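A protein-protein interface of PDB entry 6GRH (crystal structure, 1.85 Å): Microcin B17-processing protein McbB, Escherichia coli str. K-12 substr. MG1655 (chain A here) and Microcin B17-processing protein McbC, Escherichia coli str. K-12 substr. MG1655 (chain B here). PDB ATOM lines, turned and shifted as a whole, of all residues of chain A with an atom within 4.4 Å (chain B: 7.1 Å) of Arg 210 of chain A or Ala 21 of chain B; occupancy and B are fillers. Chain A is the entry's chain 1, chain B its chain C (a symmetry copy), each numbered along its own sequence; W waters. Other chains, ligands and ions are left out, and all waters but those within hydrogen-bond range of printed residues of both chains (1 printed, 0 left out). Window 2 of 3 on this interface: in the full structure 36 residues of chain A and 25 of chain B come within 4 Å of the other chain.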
ATOM      1  N   ARG A 199     -18.585  14.913  26.869  1.00  0.00           N
ATOM      2  CA  ARG A 199     -19.485  14.891  25.708  1.00  0.00           C
ATOM      3  C   ARG A 199     -19.705  16.316  25.155  1.00  0.00           C
ATOM      4  O   ARG A 199     -19.591  16.518  23.932  1.00  0.00           O
ATOM      5  CB  ARG A 199     -20.810  14.213  26.047  1.00  0.00           C
ATOM      6  CG  ARG A 199     -21.778  14.043  24.881  1.00  0.00           C
ATOM      7  CD  ARG A 199     -21.350  12.926  23.967  1.00  0.00           C
ATOM      8  NE  ARG A 199     -22.254  12.755  22.834  1.00  0.00           N
ATOM      9  CZ  ARG A 199     -22.173  13.391  21.657  1.00  0.00           C
ATOM     10  NH1 ARG A 199     -21.238  14.316  21.393  1.00  0.00           N
ATOM     11  NH2 ARG A 199     -23.071  13.101  20.725  1.00  0.00           N
ATOM     12  N   SER A 202     -16.317  17.915  23.650  1.00  0.00           N
ATOM     13  CA  SER A 202     -16.105  17.284  22.350  1.00  0.00           C
ATOM     14  C   SER A 202     -16.984  17.885  21.257  1.00  0.00           C
ATOM     15  O   SER A 202     -16.481  18.265  20.204  1.00  0.00           O
ATOM     16  CB  SER A 202     -16.358  15.768  22.437  1.00  0.00           C
ATOM     17  OG  SER A 202     -17.749  15.437  22.378  1.00  0.00           O
ATOM     18  N   ARG A 209     -16.076  15.926  13.884  1.00  0.00           N
ATOM     19  CA  ARG A 209     -15.824  14.537  14.242  1.00  0.00           C
ATOM     20  C   ARG A 209     -16.541  14.280  15.556  1.00  0.00           C
ATOM     21  O   ARG A 209     -16.525  15.133  16.447  1.00  0.00           O
ATOM     22  CB  ARG A 209     -14.323  14.278  14.411  1.00  0.00           C
ATOM     23  N   ARG A 210     -17.174  13.122  15.677  1.00  0.00           N
ATOM     24  CA  ARG A 210     -17.704  12.687  16.965  1.00  0.00           C
ATOM     25  C   ARG A 210     -16.568  12.285  17.919  1.00  0.00           C
ATOM     26  O   ARG A 210     -16.574  12.674  19.080  1.00  0.00           O
ATOM     27  CB  ARG A 210     -18.707  11.533  16.786  1.00  0.00           C
ATOM     28  CG  ARG A 210     -19.140  10.847  18.069  1.00  0.00           C
ATOM     29  CD  ARG A 210     -19.829  11.798  18.999  1.00  0.00           C
ATOM     30  NE  ARG A 210     -20.173  11.100  20.234  1.00  0.00           N
ATOM     31  CZ  ARG A 210     -19.465  11.111  21.352  1.00  0.00           C
ATOM     32  NH1 ARG A 210     -18.318  11.792  21.452  1.00  0.00           N
ATOM     33  NH2 ARG A 210     -19.910  10.404  22.393  1.00  0.00           N
ATOM     34  N   ASN A 211     -15.644  11.469  17.430  1.00  0.00           N
ATOM     35  CA  ASN A 211     -14.475  11.051  18.212  1.00  0.00           C
ATOM     36  C   ASN A 211     -13.575  12.217  18.678  1.00  0.00           C
ATOM     37  O   ASN A 211     -13.031  12.952  17.866  1.00  0.00           O
ATOM     38  CB  ASN A 211     -13.626  10.056  17.413  1.00  0.00           C
ATOM     39  CG  ASN A 211     -12.328   9.722  18.104  1.00  0.00           C
ATOM     40  OD1 ASN A 211     -12.286   9.535  19.327  1.00  0.00           O
ATOM     41  ND2 ASN A 211     -11.248   9.659  17.329  1.00  0.00           N
ATOM     42  N   GLU A 212     -13.408  12.316  19.999  1.00  0.00           N
ATOM     43  CA  GLU A 212     -12.602  13.355  20.669  1.00  0.00           C
ATOM     44  C   GLU A 212     -11.077  13.044  20.763  1.00  0.00           C
ATOM     45  O   GLU A 212     -10.283  13.950  21.047  1.00  0.00           O
ATOM     46  CB  GLU A 212     -13.189  13.642  22.082  1.00  0.00           C
ATOM     47  CG  GLU A 212     -12.737  12.782  23.284  1.00  0.00           C
ATOM     48  CD  GLU A 212     -13.326  11.359  23.356  1.00  0.00           C
ATOM     49  OE1 GLU A 212     -14.099  10.953  22.454  1.00  0.00           O
ATOM     50  OE2 GLU A 212     -13.018  10.625  24.327  1.00  0.00           O
ATOM     51  N   ILE A 285     -23.459   8.798  26.716  1.00  0.00           N
ATOM     52  CA  ILE A 285     -22.743   7.562  27.008  1.00  0.00           C
ATOM     53  C   ILE A 285     -21.696   7.787  28.110  1.00  0.00           C
ATOM     54  O   ILE A 285     -21.309   8.918  28.404  1.00  0.00           O
ATOM     55  CB  ILE A 285     -22.084   6.954  25.743  1.00  0.00           C
ATOM     56  CG1 ILE A 285     -20.992   7.853  25.164  1.00  0.00           C
ATOM     57  CG2 ILE A 285     -23.140   6.688  24.666  1.00  0.00           C
ATOM     58  CD1 ILE A 285     -20.168   7.201  24.087  1.00  0.00           C
ATOM     59  N   ASP B  16     -12.569   1.364  14.796  1.00  0.00           N
ATOM     60  CA  ASP B  16     -12.684   2.752  14.356  1.00  0.00           C
ATOM     61  C   ASP B  16     -13.424   3.505  15.472  1.00  0.00           C
ATOM     62  O   ASP B  16     -14.593   3.207  15.744  1.00  0.00           O
ATOM     63  CB  ASP B  16     -13.446   2.831  13.023  1.00  0.00           C
ATOM     64  CG  ASP B  16     -13.572   4.263  12.500  1.00  0.00           C
ATOM     65  OD1 ASP B  16     -13.587   5.216  13.310  1.00  0.00           O
ATOM     66  OD2 ASP B  16     -13.630   4.459  11.268  1.00  0.00           O
ATOM     67  N   PRO B  17     -12.750   4.468  16.133  1.00  0.00           N
ATOM     68  CA  PRO B  17     -13.346   5.112  17.313  1.00  0.00           C
ATOM     69  C   PRO B  17     -14.548   6.004  16.975  1.00  0.00           C
ATOM     70  O   PRO B  17     -15.361   6.255  17.830  1.00  0.00           O
ATOM     71  CB  PRO B  17     -12.194   5.973  17.873  1.00  0.00           C
ATOM     72  CG  PRO B  17     -11.323   6.222  16.702  1.00  0.00           C
ATOM     73  CD  PRO B  17     -11.413   5.014  15.833  1.00  0.00           C
ATOM     74  N   GLU B  18     -14.623   6.469  15.738  1.00  0.00           N
ATOM     75  CA  GLU B  18     -15.772   7.235  15.281  1.00  0.00           C
ATOM     76  C   GLU B  18     -17.004   6.320  15.181  1.00  0.00           C
ATOM     77  O   GLU B  18     -18.081   6.672  15.651  1.00  0.00           O
ATOM     78  CB  GLU B  18     -15.465   7.898  13.943  1.00  0.00           C
ATOM     79  CG  GLU B  18     -16.549   8.857  13.451  1.00  0.00           C
ATOM     80  CD  GLU B  18     -16.461  10.257  14.059  1.00  0.00           C
ATOM     81  OE1 GLU B  18     -15.557  10.528  14.892  1.00  0.00           O
ATOM     82  OE2 GLU B  18     -17.295  11.119  13.685  1.00  0.00           O
ATOM     83  N   VAL B  19     -16.822   5.139  14.596  1.00  0.00           N
ATOM     84  CA  VAL B  19     -17.899   4.175  14.470  1.00  0.00           C
ATOM     85  C   VAL B  19     -18.382   3.774  15.874  1.00  0.00           C
ATOM     86  O   VAL B  19     -19.586   3.783  16.150  1.00  0.00           O
ATOM     87  CB  VAL B  19     -17.452   2.950  13.667  1.00  0.00           C
ATOM     88  CG1 VAL B  19     -18.522   1.897  13.623  1.00  0.00           C
ATOM     89  CG2 VAL B  19     -17.125   3.364  12.237  1.00  0.00           C
ATOM     90  N   LEU B  20     -17.440   3.434  16.749  1.00  0.00           N
ATOM     91  CA  LEU B  20     -17.784   3.018  18.093  1.00  0.00           C
ATOM     92  C   LEU B  20     -18.619   4.058  18.836  1.00  0.00           C
ATOM     93  O   LEU B  20     -19.633   3.706  19.435  1.00  0.00           O
ATOM     94  CB  LEU B  20     -16.543   2.676  18.877  1.00  0.00           C
ATOM     95  CG  LEU B  20     -16.747   2.199  20.302  1.00  0.00           C
ATOM     96  CD1 LEU B  20     -17.554   0.911  20.292  1.00  0.00           C
ATOM     97  CD2 LEU B  20     -15.380   1.973  20.929  1.00  0.00           C
ATOM     98  N   ALA B  21     -18.187   5.312  18.804  1.00  0.00           N
ATOM     99  CA  ALA B  21     -18.887   6.396  19.497  1.00  0.00           C
ATOM    100  C   ALA B  21     -20.269   6.636  18.935  1.00  0.00           C
ATOM    101  O   ALA B  21     -21.214   6.775  19.691  1.00  0.00           O
ATOM    102  CB  ALA B  21     -18.075   7.689  19.445  1.00  0.00           C
ATOM    103  N   ILE B  22     -20.384   6.651  17.605  1.00  0.00           N
ATOM    104  CA  ILE B  22     -21.668   6.882  16.958  1.00  0.00           C
ATOM    105  C   ILE B  22     -22.652   5.761  17.278  1.00  0.00           C
ATOM    106  O   ILE B  22     -23.854   6.031  17.556  1.00  0.00           O
ATOM    107  CB  ILE B  22     -21.487   7.108  15.435  1.00  0.00           C
ATOM    108  CG1 ILE B  22     -20.808   8.487  15.238  1.00  0.00           C
ATOM    109  CG2 ILE B  22     -22.816   7.023  14.679  1.00  0.00           C
ATOM    110  CD1 ILE B  22     -20.361   8.821  13.818  1.00  0.00           C
ATOM    111  N   VAL B  23     -22.166   4.519  17.273  1.00  0.00           N
ATOM    112  CA  VAL B  23     -23.000   3.393  17.611  1.00  0.00           C
ATOM    113  C   VAL B  23     -23.448   3.445  19.095  1.00  0.00           C
ATOM    114  O   VAL B  23     -24.631   3.252  19.400  1.00  0.00           O
ATOM    115  CB  VAL B  23     -22.323   2.055  17.262  1.00  0.00           C
ATOM    116  CG1 VAL B  23     -23.118   0.892  17.808  1.00  0.00           C
ATOM    117  CG2 VAL B  23     -22.176   1.902  15.746  1.00  0.00           C
ATOM    118  N   LYS B  24     -22.526   3.723  20.014  1.00  0.00           N
ATOM    119  CA  LYS B  24     -22.913   3.830  21.417  1.00  0.00           C
ATOM    120  C   LYS B  24     -23.918   4.952  21.677  1.00  0.00           C
ATOM    121  O   LYS B  24     -24.853   4.785  22.474  1.00  0.00           O
ATOM    122  CB  LYS B  24     -21.696   4.033  22.301  1.00  0.00           C
ATOM    123  CG  LYS B  24     -20.795   2.824  22.484  1.00  0.00           C
ATOM    124  CD  LYS B  24     -19.538   3.361  23.189  1.00  0.00           C
ATOM    125  CE  LYS B  24     -18.744   2.308  23.858  1.00  0.00           C
ATOM    126  NZ  LYS B  24     -17.651   2.936  24.685  1.00  0.00           N
ATOM    127  N   ASP B  25     -23.695   6.102  21.030  1.00  0.00           N
ATOM    128  CA  ASP B  25     -24.583   7.231  21.141  1.00  0.00           C
ATOM    129  C   ASP B  25     -25.997   6.836  20.743  1.00  0.00           C
ATOM    130  O   ASP B  25     -26.941   7.297  21.345  1.00  0.00           O
ATOM    131  CB  ASP B  25     -24.183   8.366  20.213  1.00  0.00           C
ATOM    132  CG  ASP B  25     -22.997   9.150  20.695  1.00  0.00           C
ATOM    133  OD1 ASP B  25     -22.554   8.986  21.861  1.00  0.00           O
ATOM    134  OD2 ASP B  25     -22.512   9.978  19.858  1.00  0.00           O
ATOM    135  N   PHE B  26     -26.122   6.084  19.651  1.00  0.00           N
ATOM    136  CA  PHE B  26     -27.417   5.668  19.185  1.00  0.00           C
ATOM    137  C   PHE B  26     -28.035   4.648  20.131  1.00  0.00           C
ATOM    138  O   PHE B  26     -29.191   4.761  20.530  1.00  0.00           O
ATOM    139  CB  PHE B  26     -27.344   5.057  17.803  1.00  0.00           C
ATOM    140  CG  PHE B  26     -28.669   4.556  17.330  1.00  0.00           C
ATOM    141  CD1 PHE B  26     -29.659   5.464  16.945  1.00  0.00           C
ATOM    142  CD2 PHE B  26     -28.951   3.206  17.345  1.00  0.00           C
ATOM    143  CE1 PHE B  26     -30.902   5.016  16.502  1.00  0.00           C
ATOM    144  CE2 PHE B  26     -30.177   2.754  16.927  1.00  0.00           C
ATOM    145  CZ  PHE B  26     -31.158   3.658  16.506  1.00  0.00           C
ATOM    146  N   HIS B  27     -27.245   3.648  20.466  1.00  0.00           N
ATOM    147  CA  HIS B  27     -27.665   2.572  21.320  1.00  0.00           C
ATOM    148  C   HIS B  27     -28.324   3.060  22.631  1.00  0.00           C
ATOM    149  O   HIS B  27     -29.398   2.568  22.991  1.00  0.00           O
ATOM    150  CB  HIS B  27     -26.494   1.657  21.681  1.00  0.00           C
ATOM    151  CG  HIS B  27     -26.913   0.523  22.550  1.00  0.00           C
ATOM    152  ND1 HIS B  27     -27.454  -0.631  22.034  1.00  0.00           N
ATOM    153  CD2 HIS B  27     -26.936   0.389  23.902  1.00  0.00           C
ATOM    154  CE1 HIS B  27     -27.766  -1.442  23.031  1.00  0.00           C
ATOM    155  NE2 HIS B  27     -27.467  -0.845  24.173  1.00  0.00           N
ATOM    156  N   LEU B 199     -18.406  -4.472  15.805  1.00  0.00           N
ATOM    157  CA  LEU B 199     -18.093  -3.396  14.875  1.00  0.00           C
ATOM    158  C   LEU B 199     -16.772  -3.546  14.114  1.00  0.00           C
ATOM    159  O   LEU B 199     -16.611  -2.966  13.032  1.00  0.00           O
ATOM    160  CB  LEU B 199     -18.114  -2.053  15.619  1.00  0.00           C
ATOM    161  CG  LEU B 199     -19.489  -1.699  16.220  1.00  0.00           C
ATOM    162  CD1 LEU B 199     -19.370  -0.490  17.128  1.00  0.00           C
ATOM    163  CD2 LEU B 199     -20.510  -1.415  15.150  1.00  0.00           C
ATOM    164  N   TYR B 204     -20.611  -0.229  10.914  1.00  0.00           N
ATOM    165  CA  TYR B 204     -22.011  -0.024  11.360  1.00  0.00           C
ATOM    166  C   TYR B 204     -22.952  -1.188  11.103  1.00  0.00           C
ATOM    167  O   TYR B 204     -23.781  -1.522  11.940  1.00  0.00           O
ATOM    168  CB  TYR B 204     -22.615   1.207  10.698  1.00  0.00           C
ATOM    169  CG  TYR B 204     -21.917   2.482  11.039  1.00  0.00           C
ATOM    170  CD1 TYR B 204     -22.159   3.103  12.245  1.00  0.00           C
ATOM    171  CD2 TYR B 204     -21.012   3.076  10.149  1.00  0.00           C
ATOM    172  CE1 TYR B 204     -21.511   4.285  12.586  1.00  0.00           C
ATOM    173  CE2 TYR B 204     -20.357   4.255  10.486  1.00  0.00           C
ATOM    174  CZ  TYR B 204     -20.624   4.844  11.718  1.00  0.00           C
ATOM    175  OH  TYR B 204     -20.023   6.012  12.117  1.00  0.00           O
HETATM  176  O   HOH W   1     -23.585  10.386  23.992  1.00  0.00           O
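NE of Arg 210 of chain A lies within salt-bridge range of OD2 of Asp 25 of chain B, 2.6 Å away.
N of Arg 210 of chain A is in hydrogen-bond range of OE2 of Glu 18 of chain B (2.8 Å).
OE1 of Glu 18 of chain B sits at hydrogen-bond distance from N of Asn 211 of chain A (2.7 Å).
The guanidinium group of Arg 199 of chain A is in salt-bridge range of the side-chain carboxylate of Asp 25 of chain B (3.3 Å).
Of the printed residues of chain B, Arg 210 of chain A touches Glu 18, Ala 21 and Asp 25.
Of chain A, only Arg 210 comes within 4 Å of Ala 21 of chain B.
Of the printed residues of chain A, Lys 24 of chain B touches Ile 285.
Printed residues of chain A within 4 Å of Asp 25 of chain B: Arg 199 (3.3 Å), Arg 210 (2.6 Å) and Ile 285 (3.7 Å).
Tyr 204 of chain B touches none of the printed residues of chain A.
Ser 202 of chain A touches none of the printed residues of chain B.
Water W1 lies within hydrogen-bond range of the side-chain carboxylate of Asp 25 of chain B (2.8 Å), the guanidinium group of Arg 199 of chain A (3.0 Å) and the backbone NH of Ile 285 of chain A (3.2 Å).
OD1 of Asp 16 of chain B lies within hydrogen-bond range of N of Glu 18 of chain B (2.9 Å).
O of Arg 199 of chain A lies within hydrogen-bond range of OG of Ser 202 of chain A (2.6 Å).
Hydrophobic or aromatic side chains of chain A that line the printed part of chain B: Ile 285.
Printed residues of chain B that touch a printed residue of chain A: Pro 17, Glu 18, Ala 21, Lys 24 and Asp 25.
Among the printed residues, 9 pairs touch across the chains.
Glu 18 of chain B touches Arg 209 of chain A (OE2 to C, 3.7 Å).
Ala 21 of chain B touches Arg 210 of chain A (CB to CG, 3.6 Å).
Pro 17 of chain B touches Asn 211 of chain A.
Lys 24 of chain B touches Ile 285 of chain A (O to CG2, 3.4 Å).
OD1 of Asp 25 of chain B touches CG2 of Ile 285 of chain A, 3.7 Å away.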
